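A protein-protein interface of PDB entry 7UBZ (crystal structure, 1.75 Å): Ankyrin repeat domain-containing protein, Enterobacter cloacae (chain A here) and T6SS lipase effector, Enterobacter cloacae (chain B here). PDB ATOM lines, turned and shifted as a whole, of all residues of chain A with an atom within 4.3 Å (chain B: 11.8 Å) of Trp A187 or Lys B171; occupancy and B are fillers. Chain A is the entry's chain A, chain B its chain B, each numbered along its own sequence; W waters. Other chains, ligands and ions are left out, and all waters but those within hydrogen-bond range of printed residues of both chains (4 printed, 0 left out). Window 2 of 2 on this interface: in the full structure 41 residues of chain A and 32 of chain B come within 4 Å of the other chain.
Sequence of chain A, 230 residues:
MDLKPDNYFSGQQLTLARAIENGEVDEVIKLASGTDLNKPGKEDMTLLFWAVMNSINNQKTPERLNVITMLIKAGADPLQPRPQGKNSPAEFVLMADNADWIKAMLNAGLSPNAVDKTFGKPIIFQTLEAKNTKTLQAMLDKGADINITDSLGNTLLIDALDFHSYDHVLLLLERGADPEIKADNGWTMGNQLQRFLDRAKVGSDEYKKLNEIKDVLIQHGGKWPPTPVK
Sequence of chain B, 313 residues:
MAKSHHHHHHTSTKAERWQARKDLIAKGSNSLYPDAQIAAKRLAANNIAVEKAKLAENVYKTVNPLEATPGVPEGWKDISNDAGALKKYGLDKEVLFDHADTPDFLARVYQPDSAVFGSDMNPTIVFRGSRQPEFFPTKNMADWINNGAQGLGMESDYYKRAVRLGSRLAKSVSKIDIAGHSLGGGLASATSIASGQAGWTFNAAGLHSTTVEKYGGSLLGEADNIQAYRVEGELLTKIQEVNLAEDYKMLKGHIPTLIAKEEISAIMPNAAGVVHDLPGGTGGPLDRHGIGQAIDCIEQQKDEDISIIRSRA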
ATOM      1  N   ILE A 158      37.097  18.451  -7.577  1.00  0.00           N
ATOM      2  CA  ILE A 158      35.661  18.281  -7.389  1.00  0.00           C
ATOM      3  C   ILE A 158      34.943  18.155  -8.725  1.00  0.00           C
ATOM      4  O   ILE A 158      34.111  17.255  -8.927  1.00  0.00           O
ATOM      5  CB  ILE A 158      35.102  19.455  -6.575  1.00  0.00           C
ATOM      6  CG1 ILE A 158      35.617  19.346  -5.129  1.00  0.00           C
ATOM      7  CG2 ILE A 158      33.571  19.490  -6.673  1.00  0.00           C
ATOM      8  CD1 ILE A 158      35.256  20.622  -4.251  1.00  0.00           C
ATOM      9  N   ASP A 162      32.825  14.852 -10.584  1.00  0.00           N
ATOM     10  CA  ASP A 162      31.433  14.976 -11.012  1.00  0.00           C
ATOM     11  C   ASP A 162      31.278  14.675 -12.502  1.00  0.00           C
ATOM     12  O   ASP A 162      30.244  14.144 -12.930  1.00  0.00           O
ATOM     13  CB  ASP A 162      30.911  16.385 -10.714  1.00  0.00           C
ATOM     14  CG  ASP A 162      30.631  16.623  -9.226  1.00  0.00           C
ATOM     15  OD1 ASP A 162      30.552  15.654  -8.427  1.00  0.00           O
ATOM     16  OD2 ASP A 162      30.511  17.806  -8.839  1.00  0.00           O
ATOM     17  N   ILE A 181      39.514  20.714   0.159  1.00  0.00           N
ATOM     18  CA  ILE A 181      38.740  21.929  -0.142  1.00  0.00           C
ATOM     19  C   ILE A 181      37.246  21.636  -0.247  1.00  0.00           C
ATOM     20  O   ILE A 181      36.811  20.705  -0.936  1.00  0.00           O
ATOM     21  CB  ILE A 181      39.275  22.581  -1.429  1.00  0.00           C
ATOM     22  CG1 ILE A 181      40.688  23.099  -1.180  1.00  0.00           C
ATOM     23  CG2 ILE A 181      38.308  23.686  -1.867  1.00  0.00           C
ATOM     24  CD1 ILE A 181      41.468  23.532  -2.466  1.00  0.00           C
ATOM     25  N   LYS A 182      36.440  22.449   0.432  1.00  0.00           N
ATOM     26  CA  LYS A 182      34.991  22.373   0.350  1.00  0.00           C
ATOM     27  C   LYS A 182      34.488  23.432  -0.616  1.00  0.00           C
ATOM     28  O   LYS A 182      34.911  24.590  -0.533  1.00  0.00           O
ATOM     29  CB  LYS A 182      34.345  22.607   1.717  1.00  0.00           C
ATOM     30  CG  LYS A 182      34.806  21.617   2.765  1.00  0.00           C
ATOM     31  CD  LYS A 182      33.956  21.741   4.024  1.00  0.00           C
ATOM     32  CE  LYS A 182      34.743  22.396   5.134  1.00  0.00           C
ATOM     33  NZ  LYS A 182      33.902  22.431   6.372  1.00  0.00           N
ATOM     34  N   ALA A 183      33.556  23.047  -1.475  1.00  0.00           N
ATOM     35  CA  ALA A 183      32.879  24.013  -2.326  1.00  0.00           C
ATOM     36  C   ALA A 183      31.895  24.816  -1.483  1.00  0.00           C
ATOM     37  O   ALA A 183      31.722  24.578  -0.276  1.00  0.00           O
ATOM     38  CB  ALA A 183      32.176  23.307  -3.478  1.00  0.00           C
ATOM     39  N   ASN A 185      28.869  24.702  -1.178  1.00  0.00           N
ATOM     40  CA  ASN A 185      27.863  23.833  -0.573  1.00  0.00           C
ATOM     41  C   ASN A 185      28.433  22.947   0.538  1.00  0.00           C
ATOM     42  O   ASN A 185      27.700  22.102   1.067  1.00  0.00           O
ATOM     43  CB  ASN A 185      27.212  22.951  -1.643  1.00  0.00           C
ATOM     44  CG  ASN A 185      28.242  22.130  -2.448  1.00  0.00           C
ATOM     45  OD1 ASN A 185      29.389  21.890  -1.987  1.00  0.00           O
ATOM     46  ND2 ASN A 185      27.853  21.745  -3.667  1.00  0.00           N
ATOM     47  N   GLY A 186      29.699  23.111   0.896  1.00  0.00           N
ATOM     48  CA  GLY A 186      30.316  22.340   1.960  1.00  0.00           C
ATOM     49  C   GLY A 186      30.768  20.938   1.593  1.00  0.00           C
ATOM     50  O   GLY A 186      31.249  20.218   2.473  1.00  0.00           O
ATOM     51  N   TRP A 187      30.650  20.530   0.329  1.00  0.00           N
ATOM     52  CA  TRP A 187      31.085  19.197  -0.109  1.00  0.00           C
ATOM     53  C   TRP A 187      32.548  19.201  -0.492  1.00  0.00           C
ATOM     54  O   TRP A 187      33.039  20.148  -1.127  1.00  0.00           O
ATOM     55  CB  TRP A 187      30.284  18.709  -1.323  1.00  0.00           C
ATOM     56  CG  TRP A 187      28.920  18.280  -1.072  1.00  0.00           C
ATOM     57  CD1 TRP A 187      27.910  19.013  -0.485  1.00  0.00           C
ATOM     58  CD2 TRP A 187      28.353  17.003  -1.389  1.00  0.00           C
ATOM     59  NE1 TRP A 187      26.768  18.270  -0.436  1.00  0.00           N
ATOM     60  CE2 TRP A 187      27.017  17.021  -0.939  1.00  0.00           C
ATOM     61  CE3 TRP A 187      28.851  15.838  -2.001  1.00  0.00           C
ATOM     62  CZ2 TRP A 187      26.151  15.936  -1.113  1.00  0.00           C
ATOM     63  CZ3 TRP A 187      28.006  14.748  -2.153  1.00  0.00           C
ATOM     64  CH2 TRP A 187      26.653  14.809  -1.717  1.00  0.00           C
ATOM     65  N   THR A 188      33.245  18.125  -0.141  1.00  0.00           N
ATOM     66  CA  THR A 188      34.548  17.829  -0.719  1.00  0.00           C
ATOM     67  C   THR A 188      34.382  16.853  -1.893  1.00  0.00           C
ATOM     68  O   THR A 188      33.326  16.261  -2.105  1.00  0.00           O
ATOM     69  CB  THR A 188      35.511  17.192   0.293  1.00  0.00           C
ATOM     70  OG1 THR A 188      34.943  15.936   0.729  1.00  0.00           O
ATOM     71  CG2 THR A 188      35.787  18.125   1.520  1.00  0.00           C
ATOM     72  N   ASN A 191      33.378  13.524  -0.367  1.00  0.00           N
ATOM     73  CA  ASN A 191      31.963  13.297  -0.080  1.00  0.00           C
ATOM     74  C   ASN A 191      31.243  12.671  -1.266  1.00  0.00           C
ATOM     75  O   ASN A 191      30.425  11.753  -1.098  1.00  0.00           O
ATOM     76  CB  ASN A 191      31.258  14.598   0.295  1.00  0.00           C
ATOM     77  CG  ASN A 191      31.670  15.135   1.641  1.00  0.00           C
ATOM     78  OD1 ASN A 191      32.101  16.294   1.749  1.00  0.00           O
ATOM     79  ND2 ASN A 191      31.545  14.295   2.701  1.00  0.00           N
ATOM     80  N   GLN A 192      31.515  13.165  -2.477  1.00  0.00           N
ATOM     81  CA  GLN A 192      30.929  12.549  -3.667  1.00  0.00           C
ATOM     82  C   GLN A 192      31.531  11.167  -3.922  1.00  0.00           C
ATOM     83  O   GLN A 192      30.818  10.229  -4.301  1.00  0.00           O
ATOM     84  CB  GLN A 192      31.135  13.471  -4.886  1.00  0.00           C
ATOM     85  CG  GLN A 192      30.452  13.001  -6.170  1.00  0.00           C
ATOM     86  CD  GLN A 192      28.963  13.301  -6.131  1.00  0.00           C
ATOM     87  OE1 GLN A 192      28.217  12.638  -5.424  1.00  0.00           O
ATOM     88  NE2 GLN A 192      28.528  14.314  -6.887  1.00  0.00           N
ATOM     89  N   ARG A 195      29.700   8.629  -1.937  1.00  0.00           N
ATOM     90  CA  ARG A 195      28.418   8.306  -2.554  1.00  0.00           C
ATOM     91  C   ARG A 195      28.596   7.387  -3.759  1.00  0.00           C
ATOM     92  O   ARG A 195      27.845   6.407  -3.934  1.00  0.00           O
ATOM     93  CB  ARG A 195      27.696   9.582  -2.980  1.00  0.00           C
ATOM     94  CG  ARG A 195      26.898  10.280  -1.894  1.00  0.00           C
ATOM     95  CD  ARG A 195      25.635  10.834  -2.541  1.00  0.00           C
ATOM     96  NE  ARG A 195      25.990  11.225  -3.890  1.00  0.00           N
ATOM     97  CZ  ARG A 195      25.248  11.058  -4.974  1.00  0.00           C
ATOM     98  NH1 ARG A 195      24.009  10.619  -4.899  1.00  0.00           N
ATOM     99  NH2 ARG A 195      25.776  11.338  -6.168  1.00  0.00           N
ATOM    100  N   VAL A 229      28.964  15.970   5.333  1.00  0.00           N
ATOM    101  CA  VAL A 229      28.625  17.344   4.986  1.00  0.00           C
ATOM    102  C   VAL A 229      27.794  17.959   6.095  1.00  0.00           C
ATOM    103  O   VAL A 229      26.884  17.312   6.634  1.00  0.00           O
ATOM    104  CB  VAL A 229      27.865  17.378   3.648  1.00  0.00           C
ATOM    105  CG1 VAL A 229      27.433  18.790   3.324  1.00  0.00           C
ATOM    106  CG2 VAL A 229      28.773  16.807   2.538  1.00  0.00           C
ATOM    107  N   LEU B  86      20.395  30.550 -10.147  1.00  0.00           N
ATOM    108  CA  LEU B  86      21.001  29.234 -10.379  1.00  0.00           C
ATOM    109  C   LEU B  86      21.879  28.812  -9.218  1.00  0.00           C
ATOM    110  O   LEU B  86      22.015  27.615  -8.942  1.00  0.00           O
ATOM    111  CB  LEU B  86      21.830  29.256 -11.662  1.00  0.00           C
ATOM    112  CG  LEU B  86      20.962  29.393 -12.917  1.00  0.00           C
ATOM    113  CD1 LEU B  86      21.862  29.786 -14.125  1.00  0.00           C
ATOM    114  CD2 LEU B  86      20.247  28.064 -13.238  1.00  0.00           C
ATOM    115  N   LYS B  87      22.520  29.783  -8.573  1.00  0.00           N
ATOM    116  CA  LYS B  87      23.459  29.522  -7.495  1.00  0.00           C
ATOM    117  C   LYS B  87      22.802  28.721  -6.389  1.00  0.00           C
ATOM    118  O   LYS B  87      23.455  27.896  -5.741  1.00  0.00           O
ATOM    119  CB  LYS B  87      23.946  30.862  -6.924  1.00  0.00           C
ATOM    120  CG  LYS B  87      25.199  30.797  -6.106  1.00  0.00           C
ATOM    121  CD  LYS B  87      25.759  32.205  -5.868  1.00  0.00           C
ATOM    122  CE  LYS B  87      25.199  32.786  -4.569  1.00  0.00           C
ATOM    123  NZ  LYS B  87      25.440  34.256  -4.400  1.00  0.00           N
ATOM    124  N   LYS B  88      21.504  28.961  -6.170  1.00  0.00           N
ATOM    125  CA  LYS B  88      20.742  28.241  -5.149  1.00  0.00           C
ATOM    126  C   LYS B  88      20.844  26.731  -5.304  1.00  0.00           C
ATOM    127  O   LYS B  88      20.811  26.001  -4.308  1.00  0.00           O
ATOM    128  CB  LYS B  88      19.301  28.743  -5.226  1.00  0.00           C
ATOM    129  CG  LYS B  88      18.249  28.124  -4.348  1.00  0.00           C
ATOM    130  CD  LYS B  88      16.997  29.041  -4.367  1.00  0.00           C
ATOM    131  CE  LYS B  88      16.318  29.174  -5.745  1.00  0.00           C
ATOM    132  NZ  LYS B  88      16.826  30.258  -6.701  1.00  0.00           N
ATOM    133  N   TYR B  89      20.958  26.236  -6.538  1.00  0.00           N
ATOM    134  CA  TYR B  89      21.060  24.812  -6.840  1.00  0.00           C
ATOM    135  C   TYR B  89      22.498  24.366  -7.101  1.00  0.00           C
ATOM    136  O   TYR B  89      22.716  23.217  -7.500  1.00  0.00           O
ATOM    137  CB  TYR B  89      20.180  24.471  -8.047  1.00  0.00           C
ATOM    138  CG  TYR B  89      18.816  25.088  -7.929  1.00  0.00           C
ATOM    139  CD1 TYR B  89      17.869  24.520  -7.080  1.00  0.00           C
ATOM    140  CD2 TYR B  89      18.501  26.283  -8.557  1.00  0.00           C
ATOM    141  CE1 TYR B  89      16.589  25.087  -6.934  1.00  0.00           C
ATOM    142  CE2 TYR B  89      17.233  26.867  -8.415  1.00  0.00           C
ATOM    143  CZ  TYR B  89      16.285  26.263  -7.588  1.00  0.00           C
ATOM    144  OH  TYR B  89      15.037  26.845  -7.418  1.00  0.00           O
ATOM    145  N   GLY B  90      23.469  25.253  -6.887  1.00  0.00           N
ATOM    146  CA  GLY B  90      24.852  24.933  -7.211  1.00  0.00           C
ATOM    147  C   GLY B  90      25.142  24.950  -8.693  1.00  0.00           C
ATOM    148  O   GLY B  90      26.082  24.299  -9.141  1.00  0.00           O
ATOM    149  N   LEU B  91      24.351  25.677  -9.468  1.00  0.00           N
ATOM    150  CA  LEU B  91      24.489  25.757 -10.910  1.00  0.00           C
ATOM    151  C   LEU B  91      24.991  27.139 -11.311  1.00  0.00           C
ATOM    152  O   LEU B  91      24.902  28.097 -10.539  1.00  0.00           O
ATOM    153  CB  LEU B  91      23.161  25.487 -11.620  1.00  0.00           C
ATOM    154  CG  LEU B  91      22.513  24.110 -11.332  1.00  0.00           C
ATOM    155  CD1 LEU B  91      21.135  24.026 -11.996  1.00  0.00           C
ATOM    156  CD2 LEU B  91      23.405  22.998 -11.881  1.00  0.00           C
ATOM    157  N   VAL B  95      27.623  25.712 -17.083  1.00  0.00           N
ATOM    158  CA  VAL B  95      27.439  24.254 -17.111  1.00  0.00           C
ATOM    159  C   VAL B  95      26.166  23.824 -17.830  1.00  0.00           C
ATOM    160  O   VAL B  95      25.971  22.628 -18.043  1.00  0.00           O
ATOM    161  CB  VAL B  95      27.428  23.643 -15.692  1.00  0.00           C
ATOM    162  CG1 VAL B  95      28.703  24.054 -14.894  1.00  0.00           C
ATOM    163  CG2 VAL B  95      26.167  24.070 -14.909  1.00  0.00           C
ATOM    164  N   ILE B 125      14.959  21.066 -13.997  1.00  0.00           N
ATOM    165  CA  ILE B 125      15.944  21.244 -15.060  1.00  0.00           C
ATOM    166  C   ILE B 125      15.574  20.277 -16.175  1.00  0.00           C
ATOM    167  O   ILE B 125      15.201  19.125 -15.915  1.00  0.00           O
ATOM    168  CB  ILE B 125      17.389  21.037 -14.551  1.00  0.00           C
ATOM    169  CG1 ILE B 125      18.365  21.076 -15.735  1.00  0.00           C
ATOM    170  CG2 ILE B 125      17.534  19.659 -13.902  1.00  0.00           C
ATOM    171  CD1 ILE B 125      19.798  21.367 -15.252  1.00  0.00           C
ATOM    172  N   ALA B 162      25.927  16.034 -19.260  1.00  0.00           N
ATOM    173  CA  ALA B 162      24.704  15.573 -18.597  1.00  0.00           C
ATOM    174  C   ALA B 162      25.008  14.884 -17.266  1.00  0.00           C
ATOM    175  O   ALA B 162      24.342  15.140 -16.257  1.00  0.00           O
ATOM    176  CB  ALA B 162      23.927  14.622 -19.515  1.00  0.00           C
ATOM    177  N   VAL B 163      25.964  13.950 -17.268  1.00  0.00           N
ATOM    178  CA  VAL B 163      26.349  13.277 -16.029  1.00  0.00           C
ATOM    179  C   VAL B 163      26.860  14.290 -15.018  1.00  0.00           C
ATOM    180  O   VAL B 163      26.588  14.197 -13.814  1.00  0.00           O
ATOM    181  CB  VAL B 163      27.410  12.204 -16.345  1.00  0.00           C
ATOM    182  CG1 VAL B 163      28.108  11.718 -15.094  1.00  0.00           C
ATOM    183  CG2 VAL B 163      26.772  11.076 -17.138  1.00  0.00           C
ATOM    184  N   ARG B 164      27.657  15.255 -15.487  1.00  0.00           N
ATOM    185  CA  ARG B 164      28.196  16.249 -14.579  1.00  0.00           C
ATOM    186  C   ARG B 164      27.079  16.993 -13.841  1.00  0.00           C
ATOM    187  O   ARG B 164      27.172  17.248 -12.631  1.00  0.00           O
ATOM    188  CB  ARG B 164      29.071  17.222 -15.367  1.00  0.00           C
ATOM    189  CG  ARG B 164      29.961  18.007 -14.450  1.00  0.00           C
ATOM    190  CD  ARG B 164      29.430  19.378 -14.040  1.00  0.00           C
ATOM    191  NE  ARG B 164      29.331  20.188 -15.248  1.00  0.00           N
ATOM    192  CZ  ARG B 164      30.219  21.069 -15.683  1.00  0.00           C
ATOM    193  NH1 ARG B 164      31.268  21.448 -14.946  1.00  0.00           N
ATOM    194  NH2 ARG B 164      30.050  21.589 -16.899  1.00  0.00           N
ATOM    195  N   LEU B 165      26.016  17.359 -14.561  1.00  0.00           N
ATOM    196  CA  LEU B 165      24.879  18.035 -13.946  1.00  0.00           C
ATOM    197  C   LEU B 165      24.161  17.106 -12.967  1.00  0.00           C
ATOM    198  O   LEU B 165      23.810  17.513 -11.847  1.00  0.00           O
ATOM    199  CB  LEU B 165      23.936  18.458 -15.069  1.00  0.00           C
ATOM    200  CG  LEU B 165      24.300  19.738 -15.789  1.00  0.00           C
ATOM    201  CD1 LEU B 165      23.099  20.426 -16.440  1.00  0.00           C
ATOM    202  CD2 LEU B 165      24.951  20.709 -14.860  1.00  0.00           C
ATOM    203  N   GLY B 166      23.979  15.838 -13.348  1.00  0.00           N
ATOM    204  CA  GLY B 166      23.424  14.876 -12.401  1.00  0.00           C
ATOM    205  C   GLY B 166      24.216  14.793 -11.103  1.00  0.00           C
ATOM    206  O   GLY B 166      23.637  14.759 -10.008  1.00  0.00           O
ATOM    207  N   SER B 167      25.544  14.708 -11.210  1.00  0.00           N
ATOM    208  CA  SER B 167      26.412  14.696 -10.035  1.00  0.00           C
ATOM    209  C   SER B 167      26.210  15.948  -9.206  1.00  0.00           C
ATOM    210  O   SER B 167      26.163  15.893  -7.980  1.00  0.00           O
ATOM    211  CB  SER B 167      27.885  14.605 -10.462  1.00  0.00           C
ATOM    212  OG  SER B 167      28.138  13.398 -11.134  1.00  0.00           O
ATOM    213  N   ARG B 168      26.129  17.112  -9.860  1.00  0.00           N
ATOM    214  CA  ARG B 168      25.934  18.336  -9.097  1.00  0.00           C
ATOM    215  C   ARG B 168      24.595  18.398  -8.408  1.00  0.00           C
ATOM    216  O   ARG B 168      24.516  18.855  -7.258  1.00  0.00           O
ATOM    217  CB  ARG B 168      26.062  19.543 -10.005  1.00  0.00           C
ATOM    218  CG  ARG B 168      27.412  19.908 -10.129  1.00  0.00           C
ATOM    219  CD  ARG B 168      27.400  21.344 -10.434  1.00  0.00           C
ATOM    220  NE  ARG B 168      28.747  21.627 -10.873  1.00  0.00           N
ATOM    221  CZ  ARG B 168      29.178  22.820 -11.234  1.00  0.00           C
ATOM    222  NH1 ARG B 168      28.388  23.885 -11.168  1.00  0.00           N
ATOM    223  NH2 ARG B 168      30.412  22.932 -11.729  1.00  0.00           N
ATOM    224  N   LEU B 169      23.525  18.019  -9.109  1.00  0.00           N
ATOM    225  CA  LEU B 169      22.202  18.172  -8.515  1.00  0.00           C
ATOM    226  C   LEU B 169      22.009  17.296  -7.292  1.00  0.00           C
ATOM    227  O   LEU B 169      21.232  17.666  -6.405  1.00  0.00           O
ATOM    228  CB  LEU B 169      21.085  17.915  -9.528  1.00  0.00           C
ATOM    229  CG  LEU B 169      21.214  18.575 -10.901  1.00  0.00           C
ATOM    230  CD1 LEU B 169      20.518  17.813 -12.001  1.00  0.00           C
ATOM    231  CD2 LEU B 169      20.645  19.949 -10.805  1.00  0.00           C
ATOM    232  N   ALA B 170      22.744  16.195  -7.191  1.00  0.00           N
ATOM    233  CA  ALA B 170      22.683  15.382  -5.975  1.00  0.00           C
ATOM    234  C   ALA B 170      23.174  16.128  -4.734  1.00  0.00           C
ATOM    235  O   ALA B 170      22.819  15.742  -3.617  1.00  0.00           O
ATOM    236  CB  ALA B 170      23.492  14.101  -6.173  1.00  0.00           C
ATOM    237  N   LYS B 171      23.955  17.195  -4.886  1.00  0.00           N
ATOM    238  CA  LYS B 171      24.402  17.986  -3.754  1.00  0.00           C
ATOM    239  C   LYS B 171      23.510  19.178  -3.469  1.00  0.00           C
ATOM    240  O   LYS B 171      23.811  19.934  -2.545  1.00  0.00           O
ATOM    241  CB  LYS B 171      25.811  18.523  -4.003  1.00  0.00           C
ATOM    242  CG  LYS B 171      26.730  17.560  -4.667  1.00  0.00           C
ATOM    243  CD  LYS B 171      28.101  18.243  -4.863  1.00  0.00           C
ATOM    244  CE  LYS B 171      28.853  17.633  -6.019  1.00  0.00           C
ATOM    245  NZ  LYS B 171      30.218  18.290  -6.202  1.00  0.00           N
ATOM    246  N   SER B 172      22.455  19.400  -4.257  1.00  0.00           N
ATOM    247  CA  SER B 172      21.633  20.591  -4.063  1.00  0.00           C
ATOM    248  C   SER B 172      20.849  20.502  -2.756  1.00  0.00           C
ATOM    249  O   SER B 172      20.152  19.519  -2.523  1.00  0.00           O
ATOM    250  CB  SER B 172      20.650  20.758  -5.222  1.00  0.00           C
ATOM    251  OG  SER B 172      19.898  21.952  -5.033  1.00  0.00           O
ATOM    252  N   VAL B 173      20.907  21.560  -1.942  1.00  0.00           N
ATOM    253  CA  VAL B 173      20.051  21.605  -0.757  1.00  0.00           C
ATOM    254  C   VAL B 173      18.612  21.885  -1.160  1.00  0.00           C
ATOM    255  O   VAL B 173      17.675  21.275  -0.627  1.00  0.00           O
ATOM    256  CB  VAL B 173      20.557  22.639   0.268  1.00  0.00           C
ATOM    257  CG1 VAL B 173      21.667  22.036   1.103  1.00  0.00           C
ATOM    258  CG2 VAL B 173      21.003  23.923  -0.419  1.00  0.00           C
ATOM    259  N   SER B 174      18.408  22.784  -2.120  1.00  0.00           N
ATOM    260  CA  SER B 174      17.055  23.044  -2.588  1.00  0.00           C
ATOM    261  C   SER B 174      16.602  21.962  -3.549  1.00  0.00           C
ATOM    262  O   SER B 174      17.355  21.508  -4.424  1.00  0.00           O
ATOM    263  CB  SER B 174      16.954  24.419  -3.242  1.00  0.00           C
ATOM    264  OG  SER B 174      17.430  25.408  -2.355  1.00  0.00           O
ATOM    265  N   LYS B 175      15.353  21.545  -3.374  1.00  0.00           N
ATOM    266  CA  LYS B 175      14.786  20.503  -4.207  1.00  0.00           C
ATOM    267  C   LYS B 175      14.738  20.960  -5.663  1.00  0.00           C
ATOM    268  O   LYS B 175      14.330  22.093  -5.960  1.00  0.00           O
ATOM    269  CB  LYS B 175      13.374  20.172  -3.703  1.00  0.00           C
ATOM    270  CG  LYS B 175      12.559  19.282  -4.613  1.00  0.00           C
ATOM    271  CD  LYS B 175      13.179  17.913  -4.789  1.00  0.00           C
ATOM    272  CE  LYS B 175      12.217  16.852  -4.254  1.00  0.00           C
ATOM    273  NZ  LYS B 175      12.241  15.626  -5.089  1.00  0.00           N
ATOM    274  N   ILE B 176      15.155  20.082  -6.569  1.00  0.00           N
ATOM    275  CA  ILE B 176      15.095  20.358  -8.009  1.00  0.00           C
ATOM    276  C   ILE B 176      14.902  19.046  -8.729  1.00  0.00           C
ATOM    277  O   ILE B 176      15.634  18.088  -8.473  1.00  0.00           O
ATOM    278  CB  ILE B 176      16.356  21.103  -8.498  1.00  0.00           C
ATOM    279  CG1 ILE B 176      16.359  21.249 -10.021  1.00  0.00           C
ATOM    280  CG2 ILE B 176      17.648  20.415  -8.001  1.00  0.00           C
ATOM    281  CD1 ILE B 176      17.303  22.346 -10.453  1.00  0.00           C
ATOM    282  N   ASP B 177      13.889  18.988  -9.603  1.00  0.00           N
ATOM    283  CA  ASP B 177      13.557  17.813 -10.396  1.00  0.00           C
ATOM    284  C   ASP B 177      14.243  17.844 -11.763  1.00  0.00           C
ATOM    285  O   ASP B 177      14.527  18.905 -12.325  1.00  0.00           O
ATOM    286  CB  ASP B 177      12.052  17.715 -10.640  1.00  0.00           C
ATOM    287  CG  ASP B 177      11.273  17.383  -9.385  1.00  0.00           C
ATOM    288  OD1 ASP B 177      11.896  16.941  -8.393  1.00  0.00           O
ATOM    289  OD2 ASP B 177      10.039  17.551  -9.418  1.00  0.00           O
ATOM    290  N   ILE B 178      14.432  16.664 -12.329  1.00  0.00           N
ATOM    291  CA  ILE B 178      15.010  16.509 -13.664  1.00  0.00           C
ATOM    292  C   ILE B 178      13.944  15.982 -14.605  1.00  0.00           C
ATOM    293  O   ILE B 178      13.181  15.076 -14.250  1.00  0.00           O
ATOM    294  CB  ILE B 178      16.229  15.577 -13.667  1.00  0.00           C
ATOM    295  CG1 ILE B 178      17.295  16.107 -12.729  1.00  0.00           C
ATOM    296  CG2 ILE B 178      16.781  15.432 -15.081  1.00  0.00           C
ATOM    297  CD1 ILE B 178      18.306  15.057 -12.362  1.00  0.00           C
HETATM  298  O   HOH W   1      24.277  19.709   0.149  1.00  0.00           O
HETATM  299  O   HOH W   2      31.990  16.862  -4.467  1.00  0.00           O
HETATM  300  O   HOH W   3      30.595  19.705 -10.716  1.00  0.00           O
HETATM  301  O   HOH W   4      30.011  21.088  -5.853  1.00  0.00           O
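Of the 13 printed residues of chain A, 6 touch a printed residue of chain B.
Hydrophobic or aromatic side chains of chain A that line the printed part of chain B: Ile A158 and Trp A187.
Hydrophobic or aromatic side chains of chain B that line the printed part of chain A: Val B163 and Ala B170.
The side-chain amide oxygen of Asn A185 sits at hydrogen-bond distance from the backbone NH of Trp A187, at 3.0 Å.
The guanidinium group of Arg A195 sits at hydrogen-bond distance from the side-chain amide oxygen of Gln A192, 2.9 Å away.
O of Gly B90 lies within hydrogen-bond range of NH1 of Arg B168.
The backbone carbonyl oxygen (O) of Val B163 lies within hydrogen-bond range of the side-chain hydroxyl (OG) of Ser B167 (3.2 Å).
The backbone carbonyl oxygen (O) of Asp A162 is in hydrogen-bond range of the side-chain hydroxyl (OG) of Ser B167.
The side-chain amino group (NZ) of Lys B171 lies within salt-bridge range of the side-chain carboxylate (OD2) of Asp A162 (2.7 Å).
The backbone carbonyl oxygen of Ser B167 sits at hydrogen-bond distance from the side-chain amide nitrogen of Gln A192, at 3.0 Å.
Among the printed residues, merely in contact across the chains: Asp A162 with Arg B164, Gln A192 with Lys B171, Arg A195 with Ala B170, Ile A158 with Lys B171, Trp A187 with Lys B171, Asn A185 with Lys B171, Asp A162 with Val B163 and Asp A162 with Arg B168.
Of chain B, only Lys B171 comes within 4 Å of Trp A187.
Of chain A, only Ile A158 (3.6 Å), Asp A162 (2.7 Å), Asn A185 (3.7 Å), Trp A187 (3.6 Å) and Gln A192 (3.4 Å) come within 4 Å of Lys B171.
No residue of chain B comes within 4 Å of Ala A183.
Gly A186 touches none of the printed residues of chain B.
No residue of chain B comes within 4 Å of Thr A188.
Gln A192 touches just these residues of chain B: Ser B167 and Lys B171.
No residue of chain B comes within 4 Å of Val A229.
Printed residues of chain A within 4 Å of Val B163: Asp A162.
Printed residues of chain A within 4 Å of Arg B164: Asp A162 (3.4 Å).
The nearest printed residue of chain A that does not touch Lys B171 is Thr A188 (5.5 Å).
The nearest printed residue of chain A that does not touch Val B163 is Gln A192 (7.2 Å).
Water W3 bridges OD2 of Asp A162 (2.7 Å) and NE of Arg B168 (2.7 Å).
Water W1 bridges O of Lys B171 and NE1 of Trp A187.
Water W2 lies within hydrogen-bond range of the backbone carbonyl oxygen of Thr A188 and the side-chain amino group of Lys B171.
Water W4 lies within hydrogen-bond range of NZ of Lys B171 (2.8 Å) and ND2 of Asn A185 (3.1 Å).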
